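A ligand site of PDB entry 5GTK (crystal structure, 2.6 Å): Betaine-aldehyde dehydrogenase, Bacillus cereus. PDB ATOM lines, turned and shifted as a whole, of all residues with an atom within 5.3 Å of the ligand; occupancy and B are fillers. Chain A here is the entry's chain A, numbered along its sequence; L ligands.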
ATOM      1  N   ILE A 164      13.883  25.556 -21.267  1.00  0.00           N
ATOM      2  CA  ILE A 164      14.132  25.667 -19.828  1.00  0.00           C
ATOM      3  C   ILE A 164      14.829  26.983 -19.557  1.00  0.00           C
ATOM      4  O   ILE A 164      15.830  27.295 -20.173  1.00  0.00           O
ATOM      5  CB  ILE A 164      14.911  24.449 -19.337  1.00  0.00           C
ATOM      6  CG1 ILE A 164      14.024  23.191 -19.475  1.00  0.00           C
ATOM      7  CG2 ILE A 164      15.355  24.641 -17.891  1.00  0.00           C
ATOM      8  CD1 ILE A 164      14.803  21.908 -19.384  1.00  0.00           C
ATOM      9  N   ILE A 165      14.273  27.752 -18.646  1.00  0.00           N
ATOM     10  CA  ILE A 165      14.815  29.074 -18.320  1.00  0.00           C
ATOM     11  C   ILE A 165      15.157  29.231 -16.824  1.00  0.00           C
ATOM     12  O   ILE A 165      14.589  28.546 -15.949  1.00  0.00           O
ATOM     13  CB  ILE A 165      13.856  30.207 -18.758  1.00  0.00           C
ATOM     14  CG1 ILE A 165      12.506  30.112 -18.049  1.00  0.00           C
ATOM     15  CG2 ILE A 165      13.697  30.185 -20.264  1.00  0.00           C
ATOM     16  CD1 ILE A 165      11.525  31.208 -18.447  1.00  0.00           C
ATOM     17  N   PRO A 166      16.080  30.169 -16.526  1.00  0.00           N
ATOM     18  CA  PRO A 166      16.501  30.419 -15.184  1.00  0.00           C
ATOM     19  C   PRO A 166      15.651  31.530 -14.554  1.00  0.00           C
ATOM     20  O   PRO A 166      14.613  31.898 -15.070  1.00  0.00           O
ATOM     21  CB  PRO A 166      17.953  30.829 -15.389  1.00  0.00           C
ATOM     22  CG  PRO A 166      17.927  31.602 -16.659  1.00  0.00           C
ATOM     23  CD  PRO A 166      16.797  31.056 -17.468  1.00  0.00           C
ATOM     24  N   TRP A 167      16.151  32.068 -13.441  1.00  0.00           N
ATOM     25  CA  TRP A 167      15.384  32.877 -12.499  1.00  0.00           C
ATOM     26  C   TRP A 167      15.691  34.370 -12.477  1.00  0.00           C
ATOM     27  O   TRP A 167      14.949  35.131 -11.859  1.00  0.00           O
ATOM     28  CB  TRP A 167      15.566  32.319 -11.074  1.00  0.00           C
ATOM     29  CG  TRP A 167      16.952  31.948 -10.790  1.00  0.00           C
ATOM     30  CD1 TRP A 167      17.484  30.696 -10.852  1.00  0.00           C
ATOM     31  CD2 TRP A 167      18.020  32.829 -10.468  1.00  0.00           C
ATOM     32  NE1 TRP A 167      18.798  30.737 -10.549  1.00  0.00           N
ATOM     33  CE2 TRP A 167      19.160  32.041 -10.301  1.00  0.00           C
ATOM     34  CE3 TRP A 167      18.099  34.192 -10.221  1.00  0.00           C
ATOM     35  CZ2 TRP A 167      20.406  32.576  -9.953  1.00  0.00           C
ATOM     36  CZ3 TRP A 167      19.307  34.740  -9.879  1.00  0.00           C
ATOM     37  CH2 TRP A 167      20.458  33.939  -9.753  1.00  0.00           C
ATOM     38  N   ASN A 168      16.750  34.789 -13.136  1.00  0.00           N
ATOM     39  CA  ASN A 168      17.209  36.152 -12.981  1.00  0.00           C
ATOM     40  C   ASN A 168      16.446  37.258 -13.768  1.00  0.00           C
ATOM     41  O   ASN A 168      16.425  38.444 -13.340  1.00  0.00           O
ATOM     42  CB  ASN A 168      18.725  36.208 -13.192  1.00  0.00           C
ATOM     43  CG  ASN A 168      19.143  35.865 -14.588  1.00  0.00           C
ATOM     44  OD1 ASN A 168      18.670  34.886 -15.175  1.00  0.00           O
ATOM     45  ND2 ASN A 168      20.064  36.643 -15.139  1.00  0.00           N
ATOM     46  N   MET A 173      13.052  36.406 -20.230  1.00  0.00           N
ATOM     47  CA  MET A 173      13.619  35.171 -20.737  1.00  0.00           C
ATOM     48  C   MET A 173      12.614  34.188 -21.320  1.00  0.00           C
ATOM     49  O   MET A 173      12.906  33.504 -22.294  1.00  0.00           O
ATOM     50  CB  MET A 173      14.426  34.476 -19.657  1.00  0.00           C
ATOM     51  CG  MET A 173      15.701  35.226 -19.495  1.00  0.00           C
ATOM     52  SD  MET A 173      16.794  34.522 -18.291  1.00  0.00           S
ATOM     53  CE  MET A 173      18.367  35.016 -19.052  1.00  0.00           C
ATOM     54  N   LYS A 191       9.622  25.216 -18.949  1.00  0.00           N
ATOM     55  CA  LYS A 191       9.787  25.102 -17.519  1.00  0.00           C
ATOM     56  C   LYS A 191      10.405  26.372 -17.015  1.00  0.00           C
ATOM     57  O   LYS A 191      11.571  26.637 -17.312  1.00  0.00           O
ATOM     58  CB  LYS A 191      10.673  23.942 -17.098  1.00  0.00           C
ATOM     59  CG  LYS A 191      10.505  23.661 -15.596  1.00  0.00           C
ATOM     60  CD  LYS A 191      11.612  22.844 -14.968  1.00  0.00           C
ATOM     61  CE  LYS A 191      12.816  23.682 -14.675  1.00  0.00           C
ATOM     62  NZ  LYS A 191      12.607  24.399 -13.388  1.00  0.00           N
ATOM     63  N   PRO A 192       9.650  27.163 -16.250  1.00  0.00           N
ATOM     64  CA  PRO A 192      10.278  28.252 -15.556  1.00  0.00           C
ATOM     65  C   PRO A 192      11.103  27.763 -14.333  1.00  0.00           C
ATOM     66  O   PRO A 192      10.970  26.607 -13.877  1.00  0.00           O
ATOM     67  CB  PRO A 192       9.110  29.096 -15.099  1.00  0.00           C
ATOM     68  CG  PRO A 192       8.045  28.078 -14.860  1.00  0.00           C
ATOM     69  CD  PRO A 192       8.204  27.110 -16.000  1.00  0.00           C
ATOM     70  N   ALA A 193      11.945  28.661 -13.811  1.00  0.00           N
ATOM     71  CA  ALA A 193      12.850  28.346 -12.700  1.00  0.00           C
ATOM     72  C   ALA A 193      12.042  28.154 -11.433  1.00  0.00           C
ATOM     73  O   ALA A 193      11.124  28.906 -11.179  1.00  0.00           O
ATOM     74  CB  ALA A 193      13.852  29.465 -12.521  1.00  0.00           C
ATOM     75  N   GLU A 194      12.372  27.124 -10.664  1.00  0.00           N
ATOM     76  CA  GLU A 194      11.696  26.877  -9.369  1.00  0.00           C
ATOM     77  C   GLU A 194      11.712  28.079  -8.406  1.00  0.00           C
ATOM     78  O   GLU A 194      10.838  28.186  -7.562  1.00  0.00           O
ATOM     79  CB  GLU A 194      12.281  25.653  -8.664  1.00  0.00           C
ATOM     80  CG  GLU A 194      13.771  25.732  -8.386  1.00  0.00           C
ATOM     81  CD  GLU A 194      14.638  25.023  -9.414  1.00  0.00           C
ATOM     82  OE1 GLU A 194      14.621  25.411 -10.597  1.00  0.00           O
ATOM     83  OE2 GLU A 194      15.332  24.063  -9.005  1.00  0.00           O
ATOM     84  N   GLN A 195      12.672  28.997  -8.531  1.00  0.00           N
ATOM     85  CA  GLN A 195      12.700  30.192  -7.709  1.00  0.00           C
ATOM     86  C   GLN A 195      11.653  31.289  -8.118  1.00  0.00           C
ATOM     87  O   GLN A 195      11.317  32.141  -7.296  1.00  0.00           O
ATOM     88  CB  GLN A 195      14.106  30.808  -7.717  1.00  0.00           C
ATOM     89  CG  GLN A 195      15.213  29.876  -7.252  1.00  0.00           C
ATOM     90  CD  GLN A 195      15.767  28.980  -8.361  1.00  0.00           C
ATOM     91  OE1 GLN A 195      15.143  28.764  -9.413  1.00  0.00           O
ATOM     92  NE2 GLN A 195      16.926  28.440  -8.124  1.00  0.00           N
ATOM     93  N   GLY A 222       8.502  23.505 -11.823  1.00  0.00           N
ATOM     94  CA  GLY A 222       9.038  22.551 -10.880  1.00  0.00           C
ATOM     95  C   GLY A 222      10.545  22.489 -10.883  1.00  0.00           C
ATOM     96  O   GLY A 222      11.203  23.474 -11.199  1.00  0.00           O
ATOM     97  N   PHE A 223      11.065  21.323 -10.526  1.00  0.00           N
ATOM     98  CA  PHE A 223      12.488  21.167 -10.190  1.00  0.00           C
ATOM     99  C   PHE A 223      13.320  20.648 -11.355  1.00  0.00           C
ATOM    100  O   PHE A 223      12.816  19.961 -12.194  1.00  0.00           O
ATOM    101  CB  PHE A 223      12.645  20.386  -8.879  1.00  0.00           C
ATOM    102  CG  PHE A 223      12.330  21.218  -7.682  1.00  0.00           C
ATOM    103  CD1 PHE A 223      13.298  22.104  -7.147  1.00  0.00           C
ATOM    104  CD2 PHE A 223      11.040  21.238  -7.130  1.00  0.00           C
ATOM    105  CE1 PHE A 223      13.006  22.951  -6.075  1.00  0.00           C
ATOM    106  CE2 PHE A 223      10.754  22.089  -6.043  1.00  0.00           C
ATOM    107  CZ  PHE A 223      11.727  22.945  -5.521  1.00  0.00           C
ATOM    108  N   GLY A 224      14.584  21.086 -11.425  1.00  0.00           N
ATOM    109  CA  GLY A 224      15.500  20.714 -12.487  1.00  0.00           C
ATOM    110  C   GLY A 224      15.632  19.211 -12.664  1.00  0.00           C
ATOM    111  O   GLY A 224      15.390  18.712 -13.766  1.00  0.00           O
ATOM    112  N   PRO A 225      15.980  18.473 -11.575  1.00  0.00           N
ATOM    113  CA  PRO A 225      16.221  17.013 -11.728  1.00  0.00           C
ATOM    114  C   PRO A 225      15.021  16.157 -12.063  1.00  0.00           C
ATOM    115  O   PRO A 225      15.211  15.010 -12.473  1.00  0.00           O
ATOM    116  CB  PRO A 225      16.792  16.600 -10.381  1.00  0.00           C
ATOM    117  CG  PRO A 225      17.396  17.889  -9.844  1.00  0.00           C
ATOM    118  CD  PRO A 225      16.405  18.934 -10.243  1.00  0.00           C
ATOM    119  N   GLY A 228      12.632  19.455 -15.491  1.00  0.00           N
ATOM    120  CA  GLY A 228      13.627  19.802 -16.474  1.00  0.00           C
ATOM    121  C   GLY A 228      14.221  18.582 -17.135  1.00  0.00           C
ATOM    122  O   GLY A 228      14.259  18.508 -18.373  1.00  0.00           O
ATOM    123  N   ALA A 229      14.664  17.612 -16.343  1.00  0.00           N
ATOM    124  CA  ALA A 229      15.266  16.383 -16.881  1.00  0.00           C
ATOM    125  C   ALA A 229      14.287  15.610 -17.770  1.00  0.00           C
ATOM    126  O   ALA A 229      14.652  15.084 -18.829  1.00  0.00           O
ATOM    127  CB  ALA A 229      15.784  15.483 -15.756  1.00  0.00           C
ATOM    128  N   VAL A 232      14.396  17.305 -21.059  1.00  0.00           N
ATOM    129  CA  VAL A 232      15.670  17.020 -21.723  1.00  0.00           C
ATOM    130  C   VAL A 232      15.673  15.641 -22.401  1.00  0.00           C
ATOM    131  O   VAL A 232      16.294  15.484 -23.491  1.00  0.00           O
ATOM    132  CB  VAL A 232      16.863  17.122 -20.704  1.00  0.00           C
ATOM    133  CG1 VAL A 232      18.184  16.674 -21.330  1.00  0.00           C
ATOM    134  CG2 VAL A 232      17.048  18.543 -20.155  1.00  0.00           C
ATOM    135  N   PHE A 242      17.977  26.042 -23.900  1.00  0.00           N
ATOM    136  CA  PHE A 242      18.343  26.202 -22.501  1.00  0.00           C
ATOM    137  C   PHE A 242      19.144  27.470 -22.256  1.00  0.00           C
ATOM    138  O   PHE A 242      20.019  27.860 -23.015  1.00  0.00           O
ATOM    139  CB  PHE A 242      19.177  24.992 -22.031  1.00  0.00           C
ATOM    140  CG  PHE A 242      19.711  25.150 -20.634  1.00  0.00           C
ATOM    141  CD1 PHE A 242      18.890  24.951 -19.556  1.00  0.00           C
ATOM    142  CD2 PHE A 242      21.029  25.497 -20.408  1.00  0.00           C
ATOM    143  CE1 PHE A 242      19.372  25.061 -18.267  1.00  0.00           C
ATOM    144  CE2 PHE A 242      21.513  25.630 -19.127  1.00  0.00           C
ATOM    145  CZ  PHE A 242      20.682  25.380 -18.049  1.00  0.00           C
ATOM    146  N   THR A 243      18.825  28.092 -21.127  1.00  0.00           N
ATOM    147  CA  THR A 243      19.645  29.135 -20.610  1.00  0.00           C
ATOM    148  C   THR A 243      19.812  28.943 -19.100  1.00  0.00           C
ATOM    149  O   THR A 243      18.841  28.841 -18.368  1.00  0.00           O
ATOM    150  CB  THR A 243      19.156  30.555 -21.067  1.00  0.00           C
ATOM    151  OG1 THR A 243      19.793  31.570 -20.277  1.00  0.00           O
ATOM    152  CG2 THR A 243      17.715  30.726 -20.949  1.00  0.00           C
ATOM    153  N   GLY A 244      21.057  28.802 -18.656  1.00  0.00           N
ATOM    154  CA  GLY A 244      21.367  28.573 -17.238  1.00  0.00           C
ATOM    155  C   GLY A 244      22.848  28.366 -16.984  1.00  0.00           C
ATOM    156  O   GLY A 244      23.671  28.982 -17.648  1.00  0.00           O
ATOM    157  N   SER A 245      23.179  27.533 -16.011  1.00  0.00           N
ATOM    158  CA  SER A 245      24.579  27.286 -15.612  1.00  0.00           C
ATOM    159  C   SER A 245      25.310  26.385 -16.622  1.00  0.00           C
ATOM    160  O   SER A 245      24.683  25.548 -17.292  1.00  0.00           O
ATOM    161  CB  SER A 245      24.620  26.638 -14.228  1.00  0.00           C
ATOM    162  OG  SER A 245      24.169  25.296 -14.276  1.00  0.00           O
ATOM    163  N   THR A 248      24.803  22.454 -16.013  1.00  0.00           N
ATOM    164  CA  THR A 248      23.518  21.939 -16.467  1.00  0.00           C
ATOM    165  C   THR A 248      23.451  21.947 -18.009  1.00  0.00           C
ATOM    166  O   THR A 248      22.874  21.030 -18.612  1.00  0.00           O
ATOM    167  CB  THR A 248      22.362  22.761 -15.872  1.00  0.00           C
ATOM    168  OG1 THR A 248      22.541  22.862 -14.450  1.00  0.00           O
ATOM    169  CG2 THR A 248      20.981  22.132 -16.145  1.00  0.00           C
ATOM    170  N   TYR A 251      25.166  18.753 -19.266  1.00  0.00           N
ATOM    171  CA  TYR A 251      24.233  17.635 -19.076  1.00  0.00           C
ATOM    172  C   TYR A 251      23.211  17.566 -20.227  1.00  0.00           C
ATOM    173  O   TYR A 251      23.000  16.520 -20.800  1.00  0.00           O
ATOM    174  CB  TYR A 251      23.564  17.679 -17.684  1.00  0.00           C
ATOM    175  CG  TYR A 251      22.381  16.738 -17.565  1.00  0.00           C
ATOM    176  CD1 TYR A 251      22.567  15.360 -17.370  1.00  0.00           C
ATOM    177  CD2 TYR A 251      21.061  17.213 -17.712  1.00  0.00           C
ATOM    178  CE1 TYR A 251      21.487  14.500 -17.301  1.00  0.00           C
ATOM    179  CE2 TYR A 251      19.979  16.353 -17.628  1.00  0.00           C
ATOM    180  CZ  TYR A 251      20.206  15.003 -17.420  1.00  0.00           C
ATOM    181  OH  TYR A 251      19.134  14.129 -17.364  1.00  0.00           O
ATOM    182  N   ILE A 252      22.618  18.717 -20.567  1.00  0.00           N
ATOM    183  CA  ILE A 252      21.588  18.849 -21.615  1.00  0.00           C
ATOM    184  C   ILE A 252      22.112  18.467 -23.002  1.00  0.00           C
ATOM    185  O   ILE A 252      21.465  17.694 -23.733  1.00  0.00           O
ATOM    186  CB  ILE A 252      21.030  20.289 -21.667  1.00  0.00           C
ATOM    187  CG1 ILE A 252      20.202  20.559 -20.433  1.00  0.00           C
ATOM    188  CG2 ILE A 252      20.214  20.512 -22.942  1.00  0.00           C
ATOM    189  CD1 ILE A 252      19.650  21.944 -20.347  1.00  0.00           C
ATOM    190  N   GLU A 266      22.494  29.211 -23.765  1.00  0.00           N
ATOM    191  CA  GLU A 266      22.962  30.504 -23.299  1.00  0.00           C
ATOM    192  C   GLU A 266      23.435  30.308 -21.892  1.00  0.00           C
ATOM    193  O   GLU A 266      22.651  30.040 -21.000  1.00  0.00           O
ATOM    194  CB  GLU A 266      21.826  31.524 -23.312  1.00  0.00           C
ATOM    195  CG  GLU A 266      21.280  31.844 -24.690  1.00  0.00           C
ATOM    196  CD  GLU A 266      22.079  32.925 -25.436  1.00  0.00           C
ATOM    197  OE1 GLU A 266      22.753  33.782 -24.774  1.00  0.00           O
ATOM    198  OE2 GLU A 266      22.000  32.944 -26.701  1.00  0.00           O
ATOM    199  N   LEU A 267      24.735  30.459 -21.680  1.00  0.00           N
ATOM    200  CA  LEU A 267      25.365  30.113 -20.411  1.00  0.00           C
ATOM    201  C   LEU A 267      25.975  31.365 -19.801  1.00  0.00           C
ATOM    202  O   LEU A 267      25.629  32.481 -20.202  1.00  0.00           O
ATOM    203  CB  LEU A 267      26.394  28.992 -20.642  1.00  0.00           C
ATOM    204  CG  LEU A 267      25.923  27.776 -21.481  1.00  0.00           C
ATOM    205  CD1 LEU A 267      27.060  26.775 -21.611  1.00  0.00           C
ATOM    206  CD2 LEU A 267      24.644  27.117 -20.916  1.00  0.00           C
ATOM    207  N   GLY A 268      26.881  31.210 -18.822  1.00  0.00           N
ATOM    208  CA  GLY A 268      27.450  32.357 -18.130  1.00  0.00           C
ATOM    209  C   GLY A 268      28.538  33.084 -18.898  1.00  0.00           C
ATOM    210  O   GLY A 268      28.786  32.799 -20.071  1.00  0.00           O
ATOM    211  N   CYS A 300      24.117  37.708 -16.801  1.00  0.00           N
ATOM    212  CA  CYS A 300      25.191  36.948 -17.417  1.00  0.00           C
ATOM    213  C   CYS A 300      26.151  37.752 -18.234  1.00  0.00           C
ATOM    214  O   CYS A 300      27.263  37.320 -18.399  1.00  0.00           O
ATOM    215  CB  CYS A 300      24.634  35.788 -18.227  1.00  0.00           C
ATOM    216  SG  CYS A 300      24.408  34.418 -17.066  1.00  0.00           S
ATOM    217  N   LYS A 346      20.868  29.875  -1.172  1.00  0.00           N
ATOM    218  CA  LYS A 346      21.901  29.119  -1.894  1.00  0.00           C
ATOM    219  C   LYS A 346      22.827  30.047  -2.719  1.00  0.00           C
ATOM    220  O   LYS A 346      24.054  29.955  -2.614  1.00  0.00           O
ATOM    221  CB  LYS A 346      21.207  28.115  -2.793  1.00  0.00           C
ATOM    222  CG  LYS A 346      22.073  27.120  -3.516  1.00  0.00           C
ATOM    223  CD  LYS A 346      21.246  25.859  -3.830  1.00  0.00           C
ATOM    224  CE  LYS A 346      21.231  25.498  -5.322  1.00  0.00           C
ATOM    225  NZ  LYS A 346      22.500  24.835  -5.745  1.00  0.00           N
ATOM    226  N   GLN A 347      22.228  30.940  -3.499  1.00  0.00           N
ATOM    227  CA  GLN A 347      22.997  31.920  -4.255  1.00  0.00           C
ATOM    228  C   GLN A 347      23.747  32.902  -3.361  1.00  0.00           C
ATOM    229  O   GLN A 347      24.859  33.229  -3.646  1.00  0.00           O
ATOM    230  CB  GLN A 347      22.094  32.691  -5.223  1.00  0.00           C
ATOM    231  CG  GLN A 347      21.663  31.889  -6.428  1.00  0.00           C
ATOM    232  CD  GLN A 347      22.840  31.335  -7.175  1.00  0.00           C
ATOM    233  OE1 GLN A 347      23.024  30.120  -7.255  1.00  0.00           O
ATOM    234  NE2 GLN A 347      23.693  32.220  -7.673  1.00  0.00           N
ATOM    235  N   ARG A 350      26.693  31.108  -2.269  1.00  0.00           N
ATOM    236  CA  ARG A 350      27.611  31.043  -3.394  1.00  0.00           C
ATOM    237  C   ARG A 350      28.415  32.308  -3.469  1.00  0.00           C
ATOM    238  O   ARG A 350      29.637  32.235  -3.466  1.00  0.00           O
ATOM    239  CB  ARG A 350      26.867  30.823  -4.685  1.00  0.00           C
ATOM    240  CG  ARG A 350      27.690  30.383  -5.875  1.00  0.00           C
ATOM    241  CD  ARG A 350      26.829  29.547  -6.845  1.00  0.00           C
ATOM    242  NE  ARG A 350      27.609  28.772  -7.828  1.00  0.00           N
ATOM    243  CZ  ARG A 350      28.148  29.254  -8.934  1.00  0.00           C
ATOM    244  NH1 ARG A 350      28.039  30.566  -9.294  1.00  0.00           N
ATOM    245  NH2 ARG A 350      28.827  28.418  -9.717  1.00  0.00           N
ATOM    246  N   GLU A 397      32.557  33.082 -12.876  1.00  0.00           N
ATOM    247  CA  GLU A 397      31.323  33.807 -12.728  1.00  0.00           C
ATOM    248  C   GLU A 397      30.826  33.666 -11.321  1.00  0.00           C
ATOM    249  O   GLU A 397      30.636  32.603 -10.839  1.00  0.00           O
ATOM    250  CB  GLU A 397      30.250  33.329 -13.679  1.00  0.00           C
ATOM    251  CG  GLU A 397      28.968  34.141 -13.633  1.00  0.00           C
ATOM    252  CD  GLU A 397      27.993  33.810 -14.736  1.00  0.00           C
ATOM    253  OE1 GLU A 397      27.575  32.691 -14.804  1.00  0.00           O
ATOM    254  OE2 GLU A 397      27.618  34.666 -15.481  1.00  0.00           O
ATOM    255  N   ILE A 398      30.648  34.814 -10.687  1.00  0.00           N
ATOM    256  CA  ILE A 398      30.222  34.907  -9.288  1.00  0.00           C
ATOM    257  C   ILE A 398      28.706  35.021  -9.158  1.00  0.00           C
ATOM    258  O   ILE A 398      28.096  34.392  -8.319  1.00  0.00           O
ATOM    259  CB  ILE A 398      30.936  36.097  -8.582  1.00  0.00           C
ATOM    260  CG1 ILE A 398      32.456  35.898  -8.623  1.00  0.00           C
ATOM    261  CG2 ILE A 398      30.470  36.237  -7.132  1.00  0.00           C
ATOM    262  CD1 ILE A 398      33.265  37.102  -8.154  1.00  0.00           C
ATOM    263  N   PHE A 399      28.142  35.838 -10.010  1.00  0.00           N
ATOM    264  CA  PHE A 399      26.723  36.119 -10.083  1.00  0.00           C
ATOM    265  C   PHE A 399      26.164  36.981  -8.988  1.00  0.00           C
ATOM    266  O   PHE A 399      25.065  36.831  -8.597  1.00  0.00           O
ATOM    267  CB  PHE A 399      25.903  34.872 -10.267  1.00  0.00           C
ATOM    268  CG  PHE A 399      24.882  34.967 -11.335  1.00  0.00           C
ATOM    269  CD1 PHE A 399      25.210  35.174 -12.633  1.00  0.00           C
ATOM    270  CD2 PHE A 399      23.561  34.796 -11.028  1.00  0.00           C
ATOM    271  CE1 PHE A 399      24.252  35.221 -13.597  1.00  0.00           C
ATOM    272  CE2 PHE A 399      22.592  34.845 -12.001  1.00  0.00           C
ATOM    273  CZ  PHE A 399      22.939  35.054 -13.289  1.00  0.00           C
HETATM  274  P1  LIG L   1      20.767  25.880 -13.221  1.00  0.00           P
HETATM  275  O1  LIG L   1      21.471  25.616 -14.539  1.00  0.00           O
HETATM  276  O2  LIG L   1      20.680  24.744 -12.228  1.00  0.00           O
HETATM  277  O3  LIG L   1      19.272  26.470 -13.375  1.00  0.00           O
HETATM  278  C1  LIG L   1      18.694  26.953 -14.596  1.00  0.00           C
HETATM  279  C2  LIG L   1      17.443  26.155 -14.990  1.00  0.00           C
HETATM  280  O4  LIG L   1      17.814  24.814 -15.340  1.00  0.00           O
HETATM  281  C3  LIG L   1      16.378  26.049 -13.907  1.00  0.00           C
HETATM  282  O5  LIG L   1      15.071  26.150 -14.490  1.00  0.00           O
HETATM  283  C4  LIG L   1      16.528  24.656 -13.346  1.00  0.00           C
HETATM  284  O6  LIG L   1      15.318  24.166 -12.723  1.00  0.00           O
HETATM  285  C5  LIG L   1      17.016  23.904 -14.611  1.00  0.00           C
HETATM  286  N1  LIG L   1      17.760  22.654 -14.311  1.00  0.00           N
HETATM  287  C6  LIG L   1      18.572  22.393 -13.265  1.00  0.00           C
HETATM  288  N2  LIG L   1      19.035  21.119 -13.316  1.00  0.00           N
HETATM  289  C7  LIG L   1      18.531  20.559 -14.408  1.00  0.00           C
HETATM  290  C8  LIG L   1      18.625  19.232 -15.037  1.00  0.00           C
HETATM  291  N3  LIG L   1      19.375  18.279 -14.490  1.00  0.00           N
HETATM  292  N4  LIG L   1      17.953  19.027 -16.174  1.00  0.00           N
HETATM  293  C9  LIG L   1      17.201  20.011 -16.721  1.00  0.00           C
HETATM  294  N5  LIG L   1      17.072  21.227 -16.189  1.00  0.00           N
HETATM  295  C10 LIG L   1      17.705  21.546 -15.066  1.00  0.00           C
HETATM  296  O7  LIG L   1      21.510  27.153 -12.598  1.00  0.00           O
HETATM  297  P2  LIG L   1      21.526  27.453 -10.998  1.00  0.00           P
HETATM  298  O8  LIG L   1      21.448  26.235 -10.117  1.00  0.00           O
HETATM  299  O9  LIG L   1      20.464  28.510 -10.800  1.00  0.00           O
HETATM  300  O10 LIG L   1      23.055  27.897 -10.848  1.00  0.00           O
HETATM  301  C11 LIG L   1      23.472  29.176 -10.447  1.00  0.00           C
HETATM  302  C12 LIG L   1      24.613  29.635 -11.345  1.00  0.00           C
HETATM  303  O11 LIG L   1      24.381  29.327 -12.728  1.00  0.00           O
HETATM  304  C13 LIG L   1      24.804  31.126 -11.283  1.00  0.00           C
HETATM  305  O12 LIG L   1      25.642  31.389 -10.164  1.00  0.00           O
HETATM  306  C14 LIG L   1      25.346  31.500 -12.666  1.00  0.00           C
HETATM  307  O13 LIG L   1      26.794  31.485 -12.722  1.00  0.00           O
HETATM  308  C15 LIG L   1      24.694  30.436 -13.586  1.00  0.00           C
HETATM  309  N6  LIG L   1      23.469  30.975 -14.206  1.00  0.00           N
HETATM  310  C16 LIG L   1      23.528  31.444 -15.485  1.00  0.00           C
HETATM  311  C17 LIG L   1      22.360  31.990 -16.061  1.00  0.00           C
HETATM  312  C18 LIG L   1      22.330  32.524 -17.462  1.00  0.00           C
HETATM  313  O14 LIG L   1      21.733  33.580 -17.708  1.00  0.00           O
HETATM  314  N7  LIG L   1      22.950  31.819 -18.414  1.00  0.00           N
HETATM  315  C19 LIG L   1      21.201  32.070 -15.303  1.00  0.00           C
HETATM  316  C20 LIG L   1      21.180  31.582 -13.996  1.00  0.00           C
HETATM  317  C21 LIG L   1      22.323  31.036 -13.482  1.00  0.00           C
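NZ of Lys 191 is in salt-bridge range of OE1 of Glu 194.
The side-chain hydroxyl of Ser 245 sits at hydrogen-bond distance from the side-chain hydroxyl of Thr 248 (2.9 Å).
The backbone NH (N) of Ile 165 is in hydrogen-bond range of the backbone carbonyl oxygen (O) of Lys 191.
NZ of Lys 191 lies within hydrogen-bond range of O of Gly 222 (2.8 Å).
The backbone carbonyl oxygen (O) of Ile 165 lies within hydrogen-bond range of the backbone NH (N) of Ala 193 (3.4 Å).
The backbone carbonyl oxygen of Phe 242 lies within hydrogen-bond range of the backbone NH of Glu 266 (2.9 Å).
O of Glu 266 lies close to OG1 of Thr 243 (3.3 Å).
OD1 of Asn 168 lies close to SD of Met 173, 3.7 Å away.
CG2 of Ile 164 touches O4 of the ligand, at 3.5 Å.
Pro 166 touches the ligand.
Asn 168 touches the ligand (OD1 to C19, 3.8 Å).
Met 173 touches the ligand.
Ala 193 touches the ligand (CA to O5, 3.6 Å).
C of Gly 228 touches C9 of the ligand, 3.3 Å away.
N of Ala 229 touches C9 of the ligand (3.5 Å).
CG2 of Val 232 touches C9 of the ligand, 3.7 Å away.
Phe 242 touches the ligand (CE1 to O4, 3.3 Å).
Thr 243 touches the ligand (OG1 to N7, 3.7 Å).
CE2 of Tyr 251 touches N4 of the ligand, at 3.7 Å.
N of Gly 268 touches N7 of the ligand, 3.999 Å away.
Phe 399 touches the ligand.
Hydrophobic or aromatic side chains within 4 Å of the ligand: Ile 164, Pro 166, Trp 167, Met 173, Val 232, Phe 242, Tyr 251 and Phe 399.
Of the 35 residues printed, 27 come within 4 Å of the ligand.
The side-chain carboxylate of Glu 397 sits at hydrogen-bond distance from an oxygen (O13) of the ligand, at 2.5 Å.
The side-chain carboxylate (OE1) of Glu 194 sits at hydrogen-bond distance from an oxygen (O6) of the ligand, at 2.6 Å.
An oxygen (O12) of the ligand sits at hydrogen-bond distance from the guanidinium group (NH1) of Arg 350, 2.7 Å away.
The backbone NH of Ser 245 is in hydrogen-bond range of an oxygen (O1) of the ligand.
OG of Ser 245 lies within hydrogen-bond range of O1 of the ligand (2.7 Å).
NE1 of Trp 167 lies within hydrogen-bond range of O9 of the ligand (2.8 Å).
The side-chain amino group of Lys 191 sits at hydrogen-bond distance from an oxygen (O6) of the ligand (2.8 Å).
An oxygen (O14) of the ligand lies close to the side-chain sulfur (SG) of Cys 300, at 2.9 Å.
The backbone carbonyl oxygen (O) of Ile 165 is in hydrogen-bond range of an oxygen (O5) of the ligand.
The side-chain hydroxyl (OG1) of Thr 248 is in hydrogen-bond range of an oxygen (O1) of the ligand (3.0 Å).
The backbone carbonyl oxygen (O) of Gly 244 is in hydrogen-bond range of a nitrogen (N7) of the ligand (3.0 Å).
The backbone carbonyl oxygen (O) of Glu 266 lies within hydrogen-bond range of a nitrogen (N7) of the ligand (3.2 Å).
The side-chain amide nitrogen (NE2) of Gln 347 lies within hydrogen-bond range of an oxygen (O12) of the ligand, at 3.3 Å.
O of Leu 267 is in hydrogen-bond range of N7 of the ligand (3.3 Å).
The backbone NH (N) of Gly 224 is in hydrogen-bond range of an oxygen (O6) of the ligand (3.4 Å).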
